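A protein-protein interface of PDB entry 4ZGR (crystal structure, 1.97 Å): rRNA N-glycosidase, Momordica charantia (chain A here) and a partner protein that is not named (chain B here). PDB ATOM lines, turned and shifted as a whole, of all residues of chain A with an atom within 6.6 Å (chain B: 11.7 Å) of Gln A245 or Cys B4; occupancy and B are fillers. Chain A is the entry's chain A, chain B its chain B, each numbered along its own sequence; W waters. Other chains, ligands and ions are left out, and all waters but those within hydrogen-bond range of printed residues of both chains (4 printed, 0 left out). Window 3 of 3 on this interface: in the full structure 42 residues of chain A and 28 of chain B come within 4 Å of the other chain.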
ATOM      1  N   ILE A  38       5.040 -10.854 -16.599  1.00  0.00           N
ATOM      2  CA  ILE A  38       4.402 -12.020 -16.018  1.00  0.00           C
ATOM      3  C   ILE A  38       5.540 -12.897 -15.442  1.00  0.00           C
ATOM      4  O   ILE A  38       6.457 -13.294 -16.169  1.00  0.00           O
ATOM      5  CB  ILE A  38       3.619 -12.813 -17.093  1.00  0.00           C
ATOM      6  CG1 ILE A  38       2.509 -11.949 -17.731  1.00  0.00           C
ATOM      7  CG2 ILE A  38       3.034 -14.092 -16.521  1.00  0.00           C
ATOM      8  CD1 ILE A  38       2.049 -12.468 -19.079  1.00  0.00           C
ATOM      9  N   TRP A 194      -4.712  -9.795  -6.671  1.00  0.00           N
ATOM     10  CA  TRP A 194      -3.525  -9.939  -7.505  1.00  0.00           C
ATOM     11  C   TRP A 194      -3.609 -11.152  -8.462  1.00  0.00           C
ATOM     12  O   TRP A 194      -3.367 -11.000  -9.655  1.00  0.00           O
ATOM     13  CB  TRP A 194      -2.265 -10.019  -6.643  1.00  0.00           C
ATOM     14  CG  TRP A 194      -1.019 -10.121  -7.414  1.00  0.00           C
ATOM     15  CD1 TRP A 194      -0.463  -9.158  -8.206  1.00  0.00           C
ATOM     16  CD2 TRP A 194      -0.129 -11.238  -7.455  1.00  0.00           C
ATOM     17  NE1 TRP A 194       0.721  -9.620  -8.746  1.00  0.00           N
ATOM     18  CE2 TRP A 194       0.941 -10.896  -8.304  1.00  0.00           C
ATOM     19  CE3 TRP A 194      -0.134 -12.504  -6.856  1.00  0.00           C
ATOM     20  CZ2 TRP A 194       2.005 -11.787  -8.578  1.00  0.00           C
ATOM     21  CZ3 TRP A 194       0.934 -13.386  -7.117  1.00  0.00           C
ATOM     22  CH2 TRP A 194       1.980 -13.015  -7.962  1.00  0.00           C
ATOM     23  N   THR A 195      -3.994 -12.314  -7.945  1.00  0.00           N
ATOM     24  CA  THR A 195      -4.071 -13.507  -8.796  1.00  0.00           C
ATOM     25  C   THR A 195      -5.220 -13.376  -9.817  1.00  0.00           C
ATOM     26  O   THR A 195      -5.055 -13.750 -10.990  1.00  0.00           O
ATOM     27  CB  THR A 195      -4.157 -14.845  -7.996  1.00  0.00           C
ATOM     28  OG1 THR A 195      -5.374 -14.912  -7.262  1.00  0.00           O
ATOM     29  CG2 THR A 195      -3.020 -14.967  -7.037  1.00  0.00           C
ATOM     30  N   GLN A 196      -6.352 -12.823  -9.384  1.00  0.00           N
ATOM     31  CA  GLN A 196      -7.505 -12.633 -10.293  1.00  0.00           C
ATOM     32  C   GLN A 196      -7.204 -11.594 -11.397  1.00  0.00           C
ATOM     33  O   GLN A 196      -7.546 -11.813 -12.545  1.00  0.00           O
ATOM     34  CB  GLN A 196      -8.781 -12.305  -9.514  1.00  0.00           C
ATOM     35  CG  GLN A 196      -9.989 -11.858 -10.352  1.00  0.00           C
ATOM     36  CD  GLN A 196     -10.696 -12.993 -11.095  1.00  0.00           C
ATOM     37  OE1 GLN A 196     -10.083 -13.958 -11.528  1.00  0.00           O
ATOM     38  NE2 GLN A 196     -12.000 -12.857 -11.265  1.00  0.00           N
ATOM     39  N   LEU A 197      -6.546 -10.484 -11.049  1.00  0.00           N
ATOM     40  CA  LEU A 197      -6.114  -9.495 -12.049  1.00  0.00           C
ATOM     41  C   LEU A 197      -5.133 -10.121 -13.060  1.00  0.00           C
ATOM     42  O   LEU A 197      -5.196  -9.833 -14.249  1.00  0.00           O
ATOM     43  CB  LEU A 197      -5.463  -8.273 -11.371  1.00  0.00           C
ATOM     44  CG  LEU A 197      -6.405  -7.407 -10.543  1.00  0.00           C
ATOM     45  CD1 LEU A 197      -5.592  -6.545  -9.599  1.00  0.00           C
ATOM     46  CD2 LEU A 197      -7.317  -6.580 -11.436  1.00  0.00           C
ATOM     47  N   SER A 198      -4.243 -10.992 -12.568  1.00  0.00           N
ATOM     48  CA  SER A 198      -3.276 -11.692 -13.428  1.00  0.00           C
ATOM     49  C   SER A 198      -4.017 -12.558 -14.444  1.00  0.00           C
ATOM     50  O   SER A 198      -3.710 -12.543 -15.632  1.00  0.00           O
ATOM     51  CB  SER A 198      -2.318 -12.570 -12.590  1.00  0.00           C
ATOM     52  OG  SER A 198      -1.531 -11.798 -11.674  1.00  0.00           O
ATOM     53  N   LEU A 199      -4.999 -13.293 -13.961  1.00  0.00           N
ATOM     54  CA  LEU A 199      -5.811 -14.153 -14.811  1.00  0.00           C
ATOM     55  C   LEU A 199      -6.580 -13.317 -15.858  1.00  0.00           C
ATOM     56  O   LEU A 199      -6.467 -13.570 -17.061  1.00  0.00           O
ATOM     57  CB  LEU A 199      -6.780 -14.972 -13.967  1.00  0.00           C
ATOM     58  CG  LEU A 199      -7.863 -15.754 -14.731  1.00  0.00           C
ATOM     59  CD1 LEU A 199      -7.212 -16.724 -15.709  1.00  0.00           C
ATOM     60  CD2 LEU A 199      -8.786 -16.465 -13.764  1.00  0.00           C
ATOM     61  N   GLN A 200      -7.278 -12.282 -15.405  1.00  0.00           N
ATOM     62  CA  GLN A 200      -8.091 -11.472 -16.338  1.00  0.00           C
ATOM     63  C   GLN A 200      -7.250 -10.726 -17.387  1.00  0.00           C
ATOM     64  O   GLN A 200      -7.580 -10.733 -18.559  1.00  0.00           O
ATOM     65  CB  GLN A 200      -9.019 -10.524 -15.589  1.00  0.00           C
ATOM     66  CG  GLN A 200     -10.010 -11.198 -14.665  1.00  0.00           C
ATOM     67  CD  GLN A 200     -10.855 -12.260 -15.347  1.00  0.00           C
ATOM     68  OE1 GLN A 200     -11.201 -12.146 -16.516  1.00  0.00           O
ATOM     69  NE2 GLN A 200     -11.174 -13.306 -14.620  1.00  0.00           N
ATOM     70  N   GLN A 202      -4.299 -11.612 -18.646  1.00  0.00           N
ATOM     71  CA  GLN A 202      -3.826 -12.600 -19.592  1.00  0.00           C
ATOM     72  C   GLN A 202      -4.969 -13.131 -20.456  1.00  0.00           C
ATOM     73  O   GLN A 202      -4.830 -13.199 -21.644  1.00  0.00           O
ATOM     74  CB  GLN A 202      -3.068 -13.705 -18.847  1.00  0.00           C
ATOM     75  CG  GLN A 202      -1.711 -13.162 -18.349  1.00  0.00           C
ATOM     76  CD  GLN A 202      -1.055 -14.036 -17.287  1.00  0.00           C
ATOM     77  OE1 GLN A 202      -0.778 -15.198 -17.526  1.00  0.00           O
ATOM     78  NE2 GLN A 202      -0.821 -13.480 -16.105  1.00  0.00           N
ATOM     79  N   ALA A 203      -6.099 -13.447 -19.846  1.00  0.00           N
ATOM     80  CA  ALA A 203      -7.280 -13.895 -20.584  1.00  0.00           C
ATOM     81  C   ALA A 203      -7.787 -12.840 -21.571  1.00  0.00           C
ATOM     82  O   ALA A 203      -8.258 -13.183 -22.647  1.00  0.00           O
ATOM     83  CB  ALA A 203      -8.384 -14.263 -19.625  1.00  0.00           C
ATOM     84  N   SER A 204      -7.662 -11.565 -21.215  1.00  0.00           N
ATOM     85  CA  SER A 204      -8.161 -10.474 -22.053  1.00  0.00           C
ATOM     86  C   SER A 204      -7.507 -10.330 -23.419  1.00  0.00           C
ATOM     87  O   SER A 204      -8.025  -9.601 -24.248  1.00  0.00           O
ATOM     88  CB  SER A 204      -8.031  -9.143 -21.337  1.00  0.00           C
ATOM     89  OG  SER A 204      -6.704  -8.657 -21.341  1.00  0.00           O
ATOM     90  N   GLU A 205      -6.371 -10.999 -23.641  1.00  0.00           N
ATOM     91  CA  GLU A 205      -5.704 -11.039 -24.944  1.00  0.00           C
ATOM     92  C   GLU A 205      -6.632 -11.488 -26.078  1.00  0.00           C
ATOM     93  O   GLU A 205      -6.469 -11.042 -27.196  1.00  0.00           O
ATOM     94  CB  GLU A 205      -4.493 -11.999 -24.917  1.00  0.00           C
ATOM     95  CG  GLU A 205      -3.346 -11.620 -23.987  1.00  0.00           C
ATOM     96  CD  GLU A 205      -2.433 -10.537 -24.534  1.00  0.00           C
ATOM     97  OE1 GLU A 205      -2.604 -10.085 -25.694  1.00  0.00           O
ATOM     98  OE2 GLU A 205      -1.522 -10.112 -23.787  1.00  0.00           O
ATOM     99  N   SER A 206      -7.569 -12.384 -25.789  1.00  0.00           N
ATOM    100  CA  SER A 206      -8.519 -12.879 -26.788  1.00  0.00           C
ATOM    101  C   SER A 206      -9.788 -12.018 -26.942  1.00  0.00           C
ATOM    102  O   SER A 206     -10.596 -12.304 -27.808  1.00  0.00           O
ATOM    103  CB  SER A 206      -8.932 -14.308 -26.431  1.00  0.00           C
ATOM    104  OG  SER A 206      -9.526 -14.344 -25.132  1.00  0.00           O
ATOM    105  N   GLN A 242       2.717  -9.798 -12.745  1.00  0.00           N
ATOM    106  CA  GLN A 242       1.592 -10.723 -12.640  1.00  0.00           C
ATOM    107  C   GLN A 242       2.018 -12.160 -12.374  1.00  0.00           C
ATOM    108  O   GLN A 242       3.095 -12.552 -12.785  1.00  0.00           O
ATOM    109  CB  GLN A 242       0.845 -10.821 -13.960  1.00  0.00           C
ATOM    110  CG  GLN A 242       0.534  -9.570 -14.714  1.00  0.00           C
ATOM    111  CD  GLN A 242      -0.202  -9.893 -16.003  1.00  0.00           C
ATOM    112  OE1 GLN A 242      -1.207 -10.615 -15.996  1.00  0.00           O
ATOM    113  NE2 GLN A 242       0.289  -9.355 -17.111  1.00  0.00           N
ATOM    114  N   LEU A 243       1.121 -12.926 -11.770  1.00  0.00           N
ATOM    115  CA  LEU A 243       1.232 -14.366 -11.669  1.00  0.00           C
ATOM    116  C   LEU A 243       0.971 -15.024 -13.050  1.00  0.00           C
ATOM    117  O   LEU A 243       0.028 -14.648 -13.752  1.00  0.00           O
ATOM    118  CB  LEU A 243       0.226 -14.882 -10.651  1.00  0.00           C
ATOM    119  CG  LEU A 243       0.236 -16.386 -10.362  1.00  0.00           C
ATOM    120  CD1 LEU A 243       1.495 -16.739  -9.588  1.00  0.00           C
ATOM    121  CD2 LEU A 243      -1.004 -16.849  -9.610  1.00  0.00           C
ATOM    122  N   TYR A 244       1.800 -15.997 -13.431  1.00  0.00           N
ATOM    123  CA  TYR A 244       1.532 -16.747 -14.662  1.00  0.00           C
ATOM    124  C   TYR A 244       0.189 -17.448 -14.558  1.00  0.00           C
ATOM    125  O   TYR A 244      -0.082 -18.119 -13.573  1.00  0.00           O
ATOM    126  CB  TYR A 244       2.632 -17.757 -14.979  1.00  0.00           C
ATOM    127  CG  TYR A 244       2.303 -18.593 -16.193  1.00  0.00           C
ATOM    128  CD1 TYR A 244       2.494 -18.090 -17.472  1.00  0.00           C
ATOM    129  CD2 TYR A 244       1.790 -19.879 -16.052  1.00  0.00           C
ATOM    130  CE1 TYR A 244       2.183 -18.861 -18.591  1.00  0.00           C
ATOM    131  CE2 TYR A 244       1.474 -20.656 -17.156  1.00  0.00           C
ATOM    132  CZ  TYR A 244       1.680 -20.142 -18.414  1.00  0.00           C
ATOM    133  OH  TYR A 244       1.371 -20.903 -19.512  1.00  0.00           O
ATOM    134  N   GLN A 245      -0.676 -17.233 -15.552  1.00  0.00           N
ATOM    135  CA  GLN A 245      -2.023 -17.806 -15.532  1.00  0.00           C
ATOM    136  C   GLN A 245      -2.467 -18.547 -16.815  1.00  0.00           C
ATOM    137  O   GLN A 245      -3.096 -19.569 -16.713  1.00  0.00           O
ATOM    138  CB  GLN A 245      -3.070 -16.753 -15.140  1.00  0.00           C
ATOM    139  CG  GLN A 245      -3.043 -16.294 -13.680  1.00  0.00           C
ATOM    140  CD  GLN A 245      -3.679 -17.298 -12.716  1.00  0.00           C
ATOM    141  OE1 GLN A 245      -3.524 -18.487 -12.863  1.00  0.00           O
ATOM    142  NE2 GLN A 245      -4.369 -16.809 -11.719  1.00  0.00           N
ATOM    143  N   CYS A 246      -2.135 -18.060 -18.010  1.00  0.00           N
ATOM    144  CA  CYS A 246      -2.740 -18.515 -19.286  1.00  0.00           C
ATOM    145  C   CYS A 246      -1.635 -18.852 -20.284  1.00  0.00           C
ATOM    146  O   CYS A 246      -0.654 -18.143 -20.341  1.00  0.00           O
ATOM    147  CB  CYS A 246      -3.642 -17.403 -19.851  1.00  0.00           C
ATOM    148  SG  CYS A 246      -5.107 -17.199 -18.803  1.00  0.00           S
ATOM    149  N   PRO A 247      -1.768 -19.939 -21.075  1.00  0.00           N
ATOM    150  CA  PRO A 247      -0.787 -20.379 -22.090  1.00  0.00           C
ATOM    151  C   PRO A 247      -0.233 -19.309 -23.034  1.00  0.00           C
ATOM    152  O   PRO A 247      -0.978 -18.430 -23.444  1.00  0.00           O
ATOM    153  CB  PRO A 247      -1.586 -21.409 -22.871  1.00  0.00           C
ATOM    154  CG  PRO A 247      -2.416 -22.063 -21.821  1.00  0.00           C
ATOM    155  CD  PRO A 247      -2.789 -20.972 -20.849  1.00  0.00           C
ATOM    156  N   ASN B   1      -7.899 -24.460 -18.279  1.00  0.00           N
ATOM    157  CA  ASN B   1      -8.567 -23.392 -17.542  1.00  0.00           C
ATOM    158  C   ASN B   1      -9.368 -22.548 -18.482  1.00  0.00           C
ATOM    159  O   ASN B   1      -8.862 -21.586 -19.003  1.00  0.00           O
ATOM    160  CB  ASN B   1      -7.556 -22.525 -16.829  1.00  0.00           C
ATOM    161  CG  ASN B   1      -8.192 -21.647 -15.809  1.00  0.00           C
ATOM    162  OD1 ASN B   1      -9.409 -21.536 -15.760  1.00  0.00           O
ATOM    163  ND2 ASN B   1      -7.381 -21.016 -14.986  1.00  0.00           N
ATOM    164  N   GLU B   2     -10.619 -22.920 -18.691  1.00  0.00           N
ATOM    165  CA  GLU B   2     -11.510 -22.208 -19.631  1.00  0.00           C
ATOM    166  C   GLU B   2     -11.741 -20.730 -19.297  1.00  0.00           C
ATOM    167  O   GLU B   2     -12.191 -19.966 -20.151  1.00  0.00           O
ATOM    168  CB  GLU B   2     -12.851 -22.934 -19.743  1.00  0.00           C
ATOM    169  N   GLN B   3     -11.420 -20.334 -18.067  1.00  0.00           N
ATOM    170  CA  GLN B   3     -11.306 -18.915 -17.714  1.00  0.00           C
ATOM    171  C   GLN B   3     -10.225 -18.152 -18.496  1.00  0.00           C
ATOM    172  O   GLN B   3     -10.299 -16.935 -18.577  1.00  0.00           O
ATOM    173  CB  GLN B   3     -11.103 -18.747 -16.209  1.00  0.00           C
ATOM    174  CG  GLN B   3     -12.379 -18.891 -15.401  1.00  0.00           C
ATOM    175  CD  GLN B   3     -12.183 -18.490 -13.951  1.00  0.00           C
ATOM    176  OE1 GLN B   3     -12.474 -17.354 -13.560  1.00  0.00           O
ATOM    177  NE2 GLN B   3     -11.655 -19.409 -13.148  1.00  0.00           N
ATOM    178  N   CYS B   4      -9.254 -18.842 -19.092  1.00  0.00           N
ATOM    179  CA  CYS B   4      -8.311 -18.218 -20.043  1.00  0.00           C
ATOM    180  C   CYS B   4      -8.920 -17.776 -21.379  1.00  0.00           C
ATOM    181  O   CYS B   4      -8.337 -16.944 -22.084  1.00  0.00           O
ATOM    182  CB  CYS B   4      -7.110 -19.140 -20.295  1.00  0.00           C
ATOM    183  SG  CYS B   4      -6.095 -19.271 -18.750  1.00  0.00           S
ATOM    184  N   SER B   5     -10.092 -18.320 -21.711  1.00  0.00           N
ATOM    185  CA  SER B   5     -10.781 -18.060 -22.980  1.00  0.00           C
ATOM    186  C   SER B   5     -12.222 -17.614 -22.762  1.00  0.00           C
ATOM    187  O   SER B   5     -13.155 -18.348 -23.076  1.00  0.00           O
ATOM    188  CB  SER B   5     -10.784 -19.351 -23.786  1.00  0.00           C
ATOM    189  OG  SER B   5      -9.456 -19.798 -23.984  1.00  0.00           O
ATOM    190  N   PRO B   6     -12.447 -16.429 -22.237  1.00  0.00           N
ATOM    191  CA  PRO B   6     -13.804 -15.932 -22.019  1.00  0.00           C
ATOM    192  C   PRO B   6     -14.558 -15.846 -23.324  1.00  0.00           C
ATOM    193  O   PRO B   6     -14.020 -15.398 -24.271  1.00  0.00           O
ATOM    194  CB  PRO B   6     -13.580 -14.552 -21.433  1.00  0.00           C
ATOM    195  CG  PRO B   6     -12.220 -14.170 -21.822  1.00  0.00           C
ATOM    196  CD  PRO B   6     -11.439 -15.431 -21.902  1.00  0.00           C
ATOM    197  N   GLN B   7     -15.780 -16.307 -23.360  1.00  0.00           N
ATOM    198  CA  GLN B   7     -16.536 -16.309 -24.588  1.00  0.00           C
ATOM    199  C   GLN B   7     -17.140 -14.973 -24.957  1.00  0.00           C
ATOM    200  O   GLN B   7     -17.366 -14.706 -26.084  1.00  0.00           O
ATOM    201  CB  GLN B   7     -17.529 -17.452 -24.596  1.00  0.00           C
ATOM    202  CG  GLN B   7     -16.822 -18.805 -24.699  1.00  0.00           C
ATOM    203  CD  GLN B   7     -15.802 -18.851 -25.835  1.00  0.00           C
ATOM    204  OE1 GLN B   7     -14.596 -18.770 -25.622  1.00  0.00           O
ATOM    205  NE2 GLN B   7     -16.297 -18.937 -27.048  1.00  0.00           N
ATOM    206  N   GLN B   8     -17.363 -14.126 -23.979  1.00  0.00           N
ATOM    207  CA  GLN B   8     -17.888 -12.804 -24.236  1.00  0.00           C
ATOM    208  C   GLN B   8     -17.898 -11.948 -22.981  1.00  0.00           C
ATOM    209  O   GLN B   8     -17.834 -12.461 -21.899  1.00  0.00           O
ATOM    210  CB  GLN B   8     -19.327 -12.898 -24.757  1.00  0.00           C
ATOM    211  CG  GLN B   8     -20.311 -13.477 -23.765  1.00  0.00           C
ATOM    212  CD  GLN B   8     -21.712 -13.638 -24.335  1.00  0.00           C
ATOM    213  OE1 GLN B   8     -21.952 -14.462 -25.189  1.00  0.00           O
ATOM    214  NE2 GLN B   8     -22.626 -12.845 -23.857  1.00  0.00           N
ATOM    215  N   ARG B   9     -17.985 -10.640 -23.166  1.00  0.00           N
ATOM    216  CA  ARG B   9     -18.181  -9.743 -22.036  1.00  0.00           C
ATOM    217  C   ARG B   9     -18.905  -8.502 -22.535  1.00  0.00           C
ATOM    218  O   ARG B   9     -18.523  -7.927 -23.553  1.00  0.00           O
ATOM    219  CB  ARG B   9     -16.839  -9.343 -21.411  1.00  0.00           C
ATOM    220  CG  ARG B   9     -16.962  -8.458 -20.174  1.00  0.00           C
ATOM    221  CD  ARG B   9     -17.378  -9.262 -18.963  1.00  0.00           C
ATOM    222  NE  ARG B   9     -17.766  -8.418 -17.831  1.00  0.00           N
ATOM    223  CZ  ARG B   9     -18.226  -8.883 -16.672  1.00  0.00           C
ATOM    224  NH1 ARG B   9     -18.355 -10.193 -16.463  1.00  0.00           N
ATOM    225  NH2 ARG B   9     -18.574  -8.043 -15.720  1.00  0.00           N
ATOM    226  N   TYR B  50     -16.570 -10.104 -28.358  1.00  0.00           N
ATOM    227  CA  TYR B  50     -16.423 -11.541 -28.617  1.00  0.00           C
ATOM    228  C   TYR B  50     -15.032 -11.805 -29.166  1.00  0.00           C
ATOM    229  O   TYR B  50     -14.405 -10.896 -29.697  1.00  0.00           O
ATOM    230  CB  TYR B  50     -17.473 -12.034 -29.625  1.00  0.00           C
ATOM    231  CG  TYR B  50     -18.900 -11.867 -29.185  1.00  0.00           C
ATOM    232  CD1 TYR B  50     -19.573 -10.669 -29.415  1.00  0.00           C
ATOM    233  CD2 TYR B  50     -19.597 -12.911 -28.580  1.00  0.00           C
ATOM    234  CE1 TYR B  50     -20.894 -10.509 -29.043  1.00  0.00           C
ATOM    235  CE2 TYR B  50     -20.931 -12.763 -28.206  1.00  0.00           C
ATOM    236  CZ  TYR B  50     -21.567 -11.548 -28.433  1.00  0.00           C
ATOM    237  OH  TYR B  50     -22.882 -11.354 -28.057  1.00  0.00           O
ATOM    238  N   PRO B  51     -14.553 -13.065 -29.075  1.00  0.00           N
ATOM    239  CA  PRO B  51     -13.208 -13.366 -29.590  1.00  0.00           C
ATOM    240  C   PRO B  51     -13.044 -13.361 -31.098  1.00  0.00           C
ATOM    241  O   PRO B  51     -11.927 -13.443 -31.579  1.00  0.00           O
ATOM    242  CB  PRO B  51     -12.892 -14.739 -29.014  1.00  0.00           C
ATOM    243  CG  PRO B  51     -14.171 -15.322 -28.597  1.00  0.00           C
ATOM    244  CD  PRO B  51     -15.142 -14.203 -28.355  1.00  0.00           C
HETATM  245  O   HOH W   1      -9.589 -13.407 -30.055  1.00  0.00           O
HETATM  246  O   HOH W   2     -11.685 -15.866 -25.438  1.00  0.00           O
HETATM  247  O   HOH W   3     -14.064 -14.885 -11.931  1.00  0.00           O
HETATM  248  O   HOH W   4     -12.098 -14.904 -17.901  1.00  0.00           O
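The side-chain sulfur (SG) of Cys A246 is disulfide-bonded to the side-chain sulfur (SG) of Cys B4, 2.3 Å away. O of Gln A245 lies close to SG of Cys B4 (3.6 Å).
The backbone carbonyl oxygen of Thr A195 is in hydrogen-bond range of the side-chain amide nitrogen of Gln A245 (3.2 Å). OD1 of Asn B1 lies close to N of Gln B3 (3.3 Å). The side-chain amide oxygen (OE1) of Gln A202 is in hydrogen-bond range of the backbone NH (N) of Cys A246, 3.2 Å away. O of Ala A203 lies within hydrogen-bond range of OG of Ser A206 (3.0 Å). The backbone NH of Gln A245 lies within hydrogen-bond range of the side-chain amide oxygen of Gln A202 (2.8 Å).
Leu A199 touches Gln B3. CB of Ala A203 touches O of Gln B3, at 3.5 Å. Ala A203 touches Cys B4. Ala A203 touches Pro B6 (O to CD, 3.97 Å). Ser A206 touches Pro B6. Ser A206 touches Pro B51.
Gln A245 touches just one residue of chain B: Cys B4. Cys B4 touches just these residues of chain A: Ala A203, Gln A245 and Cys A246. No residue of chain B comes within 4 Å of Thr A195. No residue of chain B comes within 4 Å of Ser A198. No residue of chain B comes within 4 Å of Gln A202. Of chain B, only Gln B3, Cys B4 and Pro B6 come within 4 Å of Ala A203. No residue of chain B comes within 4 Å of Leu A243. No residue of chain B comes within 4 Å of Tyr A244. Cys A246 touches just one residue of chain B: Cys B4 (2.3 Å). Pro A247 touches none of the printed residues of chain B. Of the printed residues of chain A, Pro B6 touches Ala A203 (3.97 Å) and Ser A206 (3.9 Å). Of the printed residues of chain A, Pro B51 touches Ser A206. The nearest residue of chain B that does not touch Gln A245 is Asn B1 (4.8 Å).
Of the 19 printed residues of chain A, 5 touch a printed residue of chain B. Hydrophobic or aromatic side chains of chain A within 4 Å of the printed part of chain B: Leu A199 and Ala A203. Printed residues of chain B that touch a printed residue of chain A: Gln B3, Cys B4, Pro B6 and Pro B51. Along chain B the printed residues that touch a printed residue of chain A span positions 3 to 51. Among the printed residues, 8 pairs touch across the chains. Among the printed residues, no Asp or Glu carboxylate lies within 4 Å of a Lys or Arg side-chain nitrogen of the other chain.
Water W2 bridges the backbone carbonyl oxygen of Pro B6 (2.7 Å) and the side-chain hydroxyl of Ser A206 (2.7 Å). Water W1 bridges the backbone carbonyl oxygen (O) of Ser A206 (2.7 Å) and the backbone carbonyl oxygen (O) of Pro B51 (2.8 Å). Water W4 bridges the backbone carbonyl oxygen (O) of Gln B3 (2.8 Å) and the side-chain amide oxygen (OE1) of Gln A200 (3.2 Å). Water W3 lies within hydrogen-bond range of NE2 of Gln A196 (3.0 Å) and OE1 of Gln B3 (3.4 Å).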
